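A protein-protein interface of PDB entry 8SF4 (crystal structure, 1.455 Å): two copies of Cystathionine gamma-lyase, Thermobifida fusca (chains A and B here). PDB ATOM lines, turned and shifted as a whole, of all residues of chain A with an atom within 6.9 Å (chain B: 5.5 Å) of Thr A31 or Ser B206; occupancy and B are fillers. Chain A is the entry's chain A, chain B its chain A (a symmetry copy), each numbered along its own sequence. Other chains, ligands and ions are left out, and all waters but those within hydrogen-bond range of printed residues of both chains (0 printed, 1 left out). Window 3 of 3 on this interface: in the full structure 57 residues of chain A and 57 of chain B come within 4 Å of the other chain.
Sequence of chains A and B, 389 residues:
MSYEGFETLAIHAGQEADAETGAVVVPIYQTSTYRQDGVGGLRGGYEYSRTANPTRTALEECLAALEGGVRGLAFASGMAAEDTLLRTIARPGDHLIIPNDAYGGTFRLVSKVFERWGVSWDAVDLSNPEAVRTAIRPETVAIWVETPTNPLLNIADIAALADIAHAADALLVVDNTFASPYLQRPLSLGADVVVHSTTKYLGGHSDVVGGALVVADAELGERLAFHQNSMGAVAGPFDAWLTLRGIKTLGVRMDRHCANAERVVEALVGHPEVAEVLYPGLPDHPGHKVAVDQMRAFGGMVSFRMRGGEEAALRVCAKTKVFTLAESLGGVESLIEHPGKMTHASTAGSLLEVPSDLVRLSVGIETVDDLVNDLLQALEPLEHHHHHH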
ATOM      1  N   ILE A  28       0.587 -10.444  23.027  1.00  0.00           N
ATOM      2  CA  ILE A  28       0.478  -9.256  23.891  1.00  0.00           C
ATOM      3  C   ILE A  28      -0.998  -8.835  23.818  1.00  0.00           C
ATOM      4  O   ILE A  28      -1.429  -8.294  22.798  1.00  0.00           O
ATOM      5  CB  ILE A  28       1.429  -8.121  23.530  1.00  0.00           C
ATOM      6  CG1 ILE A  28       2.861  -8.628  23.317  1.00  0.00           C
ATOM      7  CG2 ILE A  28       1.338  -7.045  24.552  1.00  0.00           C
ATOM      8  CD1 ILE A  28       3.810  -7.609  22.634  1.00  0.00           C
ATOM      9  N   TYR A  29      -1.742  -9.106  24.887  1.00  0.00           N
ATOM     10  CA  TYR A  29      -3.181  -8.764  24.924  1.00  0.00           C
ATOM     11  C   TYR A  29      -3.299  -7.340  25.414  1.00  0.00           C
ATOM     12  O   TYR A  29      -3.654  -7.048  26.576  1.00  0.00           O
ATOM     13  CB  TYR A  29      -3.959  -9.779  25.753  1.00  0.00           C
ATOM     14  CG  TYR A  29      -4.119 -11.141  25.137  1.00  0.00           C
ATOM     15  CD1 TYR A  29      -3.122 -12.079  25.314  1.00  0.00           C
ATOM     16  CD2 TYR A  29      -5.237 -11.442  24.389  1.00  0.00           C
ATOM     17  CE1 TYR A  29      -3.227 -13.344  24.769  1.00  0.00           C
ATOM     18  CE2 TYR A  29      -5.329 -12.720  23.851  1.00  0.00           C
ATOM     19  CZ  TYR A  29      -4.312 -13.631  24.037  1.00  0.00           C
ATOM     20  OH  TYR A  29      -4.364 -14.944  23.485  1.00  0.00           O
ATOM     21  N   GLN A  30      -2.999  -6.409  24.529  1.00  0.00           N
ATOM     22  CA  GLN A  30      -3.107  -4.983  24.789  1.00  0.00           C
ATOM     23  C   GLN A  30      -4.565  -4.544  24.629  1.00  0.00           C
ATOM     24  O   GLN A  30      -4.994  -4.074  23.577  1.00  0.00           O
ATOM     25  CB  GLN A  30      -2.129  -4.256  23.849  1.00  0.00           C
ATOM     26  CG  GLN A  30      -1.856  -2.838  24.224  1.00  0.00           C
ATOM     27  CD  GLN A  30      -1.022  -2.670  25.507  1.00  0.00           C
ATOM     28  OE1 GLN A  30       0.013  -3.309  25.716  1.00  0.00           O
ATOM     29  NE2 GLN A  30      -1.491  -1.758  26.324  1.00  0.00           N
ATOM     30  N   THR A  31      -5.347  -4.861  25.635  1.00  0.00           N
ATOM     31  CA  THR A  31      -6.799  -4.723  25.680  1.00  0.00           C
ATOM     32  C   THR A  31      -7.180  -4.324  27.089  1.00  0.00           C
ATOM     33  O   THR A  31      -6.553  -4.779  28.028  1.00  0.00           O
ATOM     34  CB  THR A  31      -7.499  -6.032  25.263  1.00  0.00           C
ATOM     35  OG1 THR A  31      -8.874  -5.733  24.947  1.00  0.00           O
ATOM     36  CG2 THR A  31      -7.410  -7.132  26.262  1.00  0.00           C
ATOM     37  N   SER A  32      -8.228  -3.564  27.228  1.00  0.00           N
ATOM     38  CA  SER A  32      -8.776  -3.318  28.572  1.00  0.00           C
ATOM     39  C   SER A  32      -9.935  -4.248  28.931  1.00  0.00           C
ATOM     40  O   SER A  32     -10.151  -4.505  30.113  1.00  0.00           O
ATOM     41  CB  SER A  32      -9.274  -1.889  28.685  1.00  0.00           C
ATOM     42  OG  SER A  32     -10.352  -1.650  27.807  1.00  0.00           O
ATOM     43  N   THR A  33     -10.664  -4.763  27.940  1.00  0.00           N
ATOM     44  CA  THR A  33     -11.944  -5.455  28.196  1.00  0.00           C
ATOM     45  C   THR A  33     -12.168  -6.549  27.168  1.00  0.00           C
ATOM     46  O   THR A  33     -11.360  -6.733  26.228  1.00  0.00           O
ATOM     47  CB  THR A  33     -13.067  -4.399  28.255  1.00  0.00           C
ATOM     48  OG1 THR A  33     -14.191  -5.084  28.866  1.00  0.00           O
ATOM     49  CG2 THR A  33     -13.376  -3.776  26.948  1.00  0.00           C
ATOM     50  N   TYR A  34     -13.225  -7.305  27.436  1.00  0.00           N
ATOM     51  CA  TYR A  34     -13.493  -8.620  26.815  1.00  0.00           C
ATOM     52  C   TYR A  34     -14.989  -8.741  26.579  1.00  0.00           C
ATOM     53  O   TYR A  34     -15.811  -8.518  27.456  1.00  0.00           O
ATOM     54  CB  TYR A  34     -13.008  -9.727  27.743  1.00  0.00           C
ATOM     55  CG  TYR A  34     -11.557  -9.567  28.112  1.00  0.00           C
ATOM     56  CD1 TYR A  34     -11.194  -8.743  29.177  1.00  0.00           C
ATOM     57  CD2 TYR A  34     -10.528 -10.197  27.451  1.00  0.00           C
ATOM     58  CE1 TYR A  34      -9.873  -8.552  29.508  1.00  0.00           C
ATOM     59  CE2 TYR A  34      -9.208 -10.028  27.762  1.00  0.00           C
ATOM     60  CZ  TYR A  34      -8.860  -9.186  28.813  1.00  0.00           C
ATOM     61  OH  TYR A  34      -7.510  -8.932  29.092  1.00  0.00           O
ATOM     62  N   TYR A  48     -12.055  -8.151  32.535  1.00  0.00           N
ATOM     63  CA  TYR A  48     -11.513  -6.777  32.600  1.00  0.00           C
ATOM     64  C   TYR A  48     -10.055  -6.860  32.941  1.00  0.00           C
ATOM     65  O   TYR A  48      -9.675  -7.602  33.881  1.00  0.00           O
ATOM     66  CB  TYR A  48     -12.278  -5.926  33.661  1.00  0.00           C
ATOM     67  CG  TYR A  48     -11.829  -4.472  33.656  1.00  0.00           C
ATOM     68  CD1 TYR A  48     -12.251  -3.677  32.621  1.00  0.00           C
ATOM     69  CD2 TYR A  48     -11.113  -3.905  34.685  1.00  0.00           C
ATOM     70  CE1 TYR A  48     -11.887  -2.346  32.543  1.00  0.00           C
ATOM     71  CE2 TYR A  48     -10.727  -2.574  34.644  1.00  0.00           C
ATOM     72  CZ  TYR A  48     -11.189  -1.799  33.613  1.00  0.00           C
ATOM     73  OH  TYR A  48     -10.890  -0.430  33.580  1.00  0.00           O
ATOM     74  N   SER A  49      -9.146  -6.164  32.260  1.00  0.00           N
ATOM     75  CA  SER A  49      -7.710  -6.457  32.373  1.00  0.00           C
ATOM     76  C   SER A  49      -7.102  -6.204  33.727  1.00  0.00           C
ATOM     77  O   SER A  49      -6.197  -6.939  34.106  1.00  0.00           O
ATOM     78  CB  SER A  49      -6.858  -5.764  31.308  1.00  0.00           C
ATOM     79  OG  SER A  49      -7.046  -6.446  30.056  1.00  0.00           O
ATOM     80  N   ARG A  50      -7.592  -5.220  34.498  1.00  0.00           N
ATOM     81  CA  ARG A  50      -7.035  -5.049  35.880  1.00  0.00           C
ATOM     82  C   ARG A  50      -7.281  -6.341  36.658  1.00  0.00           C
ATOM     83  O   ARG A  50      -6.383  -6.804  37.362  1.00  0.00           O
ATOM     84  CB  ARG A  50      -7.701  -3.849  36.548  1.00  0.00           C
ATOM     85  CG  ARG A  50      -7.327  -3.751  38.018  1.00  0.00           C
ATOM     86  CD  ARG A  50      -7.646  -2.402  38.602  1.00  0.00           C
ATOM     87  NE  ARG A  50      -8.847  -1.744  38.176  1.00  0.00           N
ATOM     88  CZ  ARG A  50     -10.084  -2.123  38.408  1.00  0.00           C
ATOM     89  NH1 ARG A  50     -11.095  -1.477  37.890  1.00  0.00           N
ATOM     90  NH2 ARG A  50     -10.311  -3.204  39.141  1.00  0.00           N
ATOM     91  N   ASN A  53      -5.594 -10.466  32.910  1.00  0.00           N
ATOM     92  CA  ASN A  53      -5.235 -10.251  31.475  1.00  0.00           C
ATOM     93  C   ASN A  53      -4.498 -11.489  31.000  1.00  0.00           C
ATOM     94  O   ASN A  53      -3.643 -11.980  31.766  1.00  0.00           O
ATOM     95  CB  ASN A  53      -4.356  -9.004  31.397  1.00  0.00           C
ATOM     96  CG  ASN A  53      -3.743  -8.792  30.025  1.00  0.00           C
ATOM     97  OD1 ASN A  53      -2.774  -9.511  29.700  1.00  0.00           O
ATOM     98  ND2 ASN A  53      -4.305  -7.839  29.263  1.00  0.00           N
ATOM     99  N   PRO A  54      -4.701 -12.007  29.774  1.00  0.00           N
ATOM    100  CA  PRO A  54      -4.114 -13.301  29.434  1.00  0.00           C
ATOM    101  C   PRO A  54      -2.574 -13.268  29.390  1.00  0.00           C
ATOM    102  O   PRO A  54      -1.959 -14.296  29.692  1.00  0.00           O
ATOM    103  CB  PRO A  54      -4.750 -13.662  28.115  1.00  0.00           C
ATOM    104  CG  PRO A  54      -6.020 -12.825  28.036  1.00  0.00           C
ATOM    105  CD  PRO A  54      -5.690 -11.569  28.798  1.00  0.00           C
ATOM    106  N   PRO A 237       0.303  -5.481  30.253  1.00  0.00           N
ATOM    107  CA  PRO A 237       0.585  -6.664  29.439  1.00  0.00           C
ATOM    108  C   PRO A 237       1.909  -6.614  28.699  1.00  0.00           C
ATOM    109  O   PRO A 237       2.606  -7.637  28.585  1.00  0.00           O
ATOM    110  CB  PRO A 237      -0.589  -6.772  28.497  1.00  0.00           C
ATOM    111  CG  PRO A 237      -1.247  -5.483  28.523  1.00  0.00           C
ATOM    112  CD  PRO A 237      -0.988  -4.869  29.892  1.00  0.00           C
ATOM    113  N   THR B 199      -7.892   4.498  31.350  1.00  0.00           N
ATOM    114  CA  THR B 199      -8.428   3.356  30.625  1.00  0.00           C
ATOM    115  C   THR B 199      -9.592   3.752  29.759  1.00  0.00           C
ATOM    116  O   THR B 199      -9.915   3.033  28.821  1.00  0.00           O
ATOM    117  CB  THR B 199      -8.888   2.374  31.674  1.00  0.00           C
ATOM    118  OG1 THR B 199      -7.853   2.105  32.635  1.00  0.00           O
ATOM    119  CG2 THR B 199      -9.325   1.067  31.072  1.00  0.00           C
ATOM    120  N   GLY B 203      -7.160   7.354  27.125  1.00  0.00           N
ATOM    121  CA  GLY B 203      -6.528   6.411  26.184  1.00  0.00           C
ATOM    122  C   GLY B 203      -7.378   6.191  24.962  1.00  0.00           C
ATOM    123  O   GLY B 203      -6.881   6.172  23.841  1.00  0.00           O
ATOM    124  N   GLY B 204      -8.690   6.016  25.177  1.00  0.00           N
ATOM    125  CA  GLY B 204      -9.704   6.119  24.141  1.00  0.00           C
ATOM    126  C   GLY B 204      -9.899   4.912  23.233  1.00  0.00           C
ATOM    127  O   GLY B 204     -10.790   5.009  22.373  1.00  0.00           O
ATOM    128  N   HIS B 205      -9.117   3.869  23.381  1.00  0.00           N
ATOM    129  CA  HIS B 205      -9.139   2.781  22.376  1.00  0.00           C
ATOM    130  C   HIS B 205      -9.246   1.398  23.040  1.00  0.00           C
ATOM    131  O   HIS B 205      -8.976   0.398  22.355  1.00  0.00           O
ATOM    132  CB  HIS B 205      -7.890   2.884  21.479  1.00  0.00           C
ATOM    133  CG  HIS B 205      -7.861   4.122  20.659  1.00  0.00           C
ATOM    134  ND1 HIS B 205      -7.545   5.355  21.214  1.00  0.00           N
ATOM    135  CD2 HIS B 205      -8.035   4.319  19.337  1.00  0.00           C
ATOM    136  CE1 HIS B 205      -7.600   6.257  20.214  1.00  0.00           C
ATOM    137  NE2 HIS B 205      -7.893   5.678  19.039  1.00  0.00           N
ATOM    138  N   SER B 206      -9.733   1.367  24.275  1.00  0.00           N
ATOM    139  CA  SER B 206      -9.968   0.079  24.972  1.00  0.00           C
ATOM    140  C   SER B 206      -8.775  -0.838  24.987  1.00  0.00           C
ATOM    141  O   SER B 206      -8.913  -2.037  24.950  1.00  0.00           O
ATOM    142  CB  SER B 206     -11.101  -0.649  24.413  1.00  0.00           C
ATOM    143  OG  SER B 206     -12.275   0.194  24.559  1.00  0.00           O
ATOM    144  N   ASP B 207      -7.543  -0.271  25.018  1.00  0.00           N
ATOM    145  CA  ASP B 207      -6.324  -1.033  24.844  1.00  0.00           C
ATOM    146  C   ASP B 207      -5.266  -0.686  25.884  1.00  0.00           C
ATOM    147  O   ASP B 207      -4.158  -1.180  25.709  1.00  0.00           O
ATOM    148  CB  ASP B 207      -5.798  -0.908  23.428  1.00  0.00           C
ATOM    149  CG  ASP B 207      -5.479   0.483  22.929  1.00  0.00           C
ATOM    150  OD1 ASP B 207      -5.421   1.414  23.802  1.00  0.00           O
ATOM    151  OD2 ASP B 207      -5.251   0.594  21.699  1.00  0.00           O
ATOM    152  N   VAL B 208      -5.552   0.096  26.918  1.00  0.00           N
ATOM    153  CA  VAL B 208      -4.587   0.408  28.001  1.00  0.00           C
ATOM    154  C   VAL B 208      -5.346   0.558  29.289  1.00  0.00           C
ATOM    155  O   VAL B 208      -6.561   1.022  29.286  1.00  0.00           O
ATOM    156  CB  VAL B 208      -3.884   1.738  27.779  1.00  0.00           C
ATOM    157  CG1 VAL B 208      -2.783   1.949  28.809  1.00  0.00           C
ATOM    158  CG2 VAL B 208      -3.257   1.893  26.591  1.00  0.00           C
ATOM    159  N   VAL B 209      -4.893  -0.048  30.333  1.00  0.00           N
ATOM    160  CA  VAL B 209      -5.397   0.223  31.674  1.00  0.00           C
ATOM    161  C   VAL B 209      -4.404   1.156  32.323  1.00  0.00           C
ATOM    162  O   VAL B 209      -3.217   0.870  32.388  1.00  0.00           O
ATOM    163  CB  VAL B 209      -5.559  -1.068  32.466  1.00  0.00           C
ATOM    164  CG1 VAL B 209      -5.812  -0.795  33.941  1.00  0.00           C
ATOM    165  CG2 VAL B 209      -6.683  -1.939  31.906  1.00  0.00           C
ATOM    166  N   LEU B 329     -15.636   1.489  29.218  1.00  0.00           N
ATOM    167  CA  LEU B 329     -16.320   2.600  28.549  1.00  0.00           C
ATOM    168  C   LEU B 329     -15.259   3.549  27.975  1.00  0.00           C
ATOM    169  O   LEU B 329     -14.067   3.392  28.310  1.00  0.00           O
ATOM    170  CB  LEU B 329     -17.270   3.355  29.490  1.00  0.00           C
ATOM    171  CG  LEU B 329     -16.585   3.966  30.715  1.00  0.00           C
ATOM    172  CD1 LEU B 329     -16.498   5.498  30.674  1.00  0.00           C
ATOM    173  CD2 LEU B 329     -17.286   3.510  31.974  1.00  0.00           C
ATOM    174  N   GLY B 330     -15.704   4.492  27.154  1.00  0.00           N
ATOM    175  CA  GLY B 330     -14.822   5.552  26.689  1.00  0.00           C
ATOM    176  C   GLY B 330     -13.956   5.169  25.527  1.00  0.00           C
ATOM    177  O   GLY B 330     -13.111   6.027  25.138  1.00  0.00           O
ATOM    178  N   GLY B 331     -14.143   4.015  24.921  1.00  0.00           N
ATOM    179  CA  GLY B 331     -13.414   3.652  23.709  1.00  0.00           C
ATOM    180  C   GLY B 331     -14.114   4.123  22.476  1.00  0.00           C
ATOM    181  O   GLY B 331     -15.317   4.442  22.436  1.00  0.00           O
ATOM    182  N   VAL B 332     -13.351   4.064  21.375  1.00  0.00           N
ATOM    183  CA  VAL B 332     -13.935   4.350  20.043  1.00  0.00           C
ATOM    184  C   VAL B 332     -15.112   3.408  19.777  1.00  0.00           C
ATOM    185  O   VAL B 332     -16.009   3.779  19.000  1.00  0.00           O
ATOM    186  CB  VAL B 332     -12.880   4.356  18.965  1.00  0.00           C
ATOM    187  CG1 VAL B 332     -11.890   5.533  19.163  1.00  0.00           C
ATOM    188  CG2 VAL B 332     -12.083   3.046  18.897  1.00  0.00           C
ATOM    189  N   GLU B 333     -14.995   2.176  20.210  1.00  0.00           N
ATOM    190  CA  GLU B 333     -15.995   1.154  19.943  1.00  0.00           C
ATOM    191  C   GLU B 333     -17.131   1.317  20.945  1.00  0.00           C
ATOM    192  O   GLU B 333     -16.920   1.539  22.170  1.00  0.00           O
ATOM    193  CB  GLU B 333     -15.390  -0.204  19.974  1.00  0.00           C
ATOM    194  CG  GLU B 333     -15.119  -0.732  21.333  1.00  0.00           C
ATOM    195  CD  GLU B 333     -14.058   0.005  22.207  1.00  0.00           C
ATOM    196  OE1 GLU B 333     -13.019   0.676  21.728  1.00  0.00           O
ATOM    197  OE2 GLU B 333     -14.256  -0.213  23.499  1.00  0.00           O
ATOM    198  N   LEU B 335     -19.924   0.173  23.556  1.00  0.00           N
ATOM    199  CA  LEU B 335     -20.080  -0.919  24.512  1.00  0.00           C
ATOM    200  C   LEU B 335     -21.450  -0.797  25.191  1.00  0.00           C
ATOM    201  O   LEU B 335     -21.994   0.303  25.350  1.00  0.00           O
ATOM    202  CB  LEU B 335     -18.989  -0.875  25.574  1.00  0.00           C
ATOM    203  CG  LEU B 335     -17.560  -0.938  25.081  1.00  0.00           C
ATOM    204  CD1 LEU B 335     -16.580  -0.802  26.229  1.00  0.00           C
ATOM    205  CD2 LEU B 335     -17.276  -2.268  24.340  1.00  0.00           C
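The backbone carbonyl oxygen of Asp B207 sits at hydrogen-bond distance from the side-chain amide nitrogen of Gln A30 (2.8 Å). N of Ser A32 lies within hydrogen-bond range of O of Ser B206, at 2.8 Å.
OG1 of Thr A31 sits at hydrogen-bond distance from O of Thr A33 (3.0 Å). O of Thr A31 sits at hydrogen-bond distance from OG of Ser A49, at 2.7 Å. O of Ser A32 is in hydrogen-bond range of N of Ser A49 (2.9 Å). The side-chain hydroxyl of Ser A49 is in hydrogen-bond range of the side-chain hydroxyl of Tyr A34. OG of Ser A49 sits at hydrogen-bond distance from ND2 of Asn A53 (3.2 Å). OG of Ser B206 sits close to OE1 of Glu B333, 3.0 Å away.
Among the printed residues, pairs that only touch across the chains: Tyr A48 with Thr B199 (3.3 Å), Thr A31 with Ser B206 (3.5 Å), Ser A32 with Thr B199 (3.8 Å), Thr A31 with Asp B207 (3.8 Å), Ser A49 with Val B209 (3.9 Å) and Ser A32 with Asp B207 (3.96 Å).
Of the printed residues of chain B, Gln A30 touches Asp B207 (2.8 Å). Of chain B, only Ser B206 (3.5 Å) and Asp B207 (3.8 Å) come within 4 Å of Thr A31. Of the printed residues of chain B, Ser A32 touches Thr B199 (3.8 Å), Ser B206 (2.8 Å) and Asp B207 (3.96 Å). Of the printed residues of chain B, Tyr A48 touches Thr B199. Of the printed residues of chain B, Ser A49 touches Val B209. Printed residues of chain A within 4 Å of Asp B207: Gln A30 (2.8 Å), Thr A31 (3.8 Å) and Ser A32 (3.96 Å). The nearest residue of chain B that does not touch Thr A31 is Val B208 (4.7 Å). The nearest residue of chain A that does not touch Ser B206 is Thr A33 (4.4 Å).
Of the 13 printed residues of chain A, 5 touch a printed residue of chain B. Printed residues of chain A that touch a printed residue of chain B: Gln A30, Thr A31, Ser A32, Tyr A48 and Ser A49. Hydrophobic or aromatic side chains of chain A that line the printed part of chain B: Tyr A48. Along chain A the printed residues that touch a printed residue of chain B span positions 30 to 49. Printed residues of chain B that touch a printed residue of chain A: Thr B199, Ser B206, Asp B207 and Val B209. Among the printed residues, no Asp or Glu carboxylate lies within 4 Å of a Lys or Arg side-chain nitrogen of the other chain.
No position is printed for both chains.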
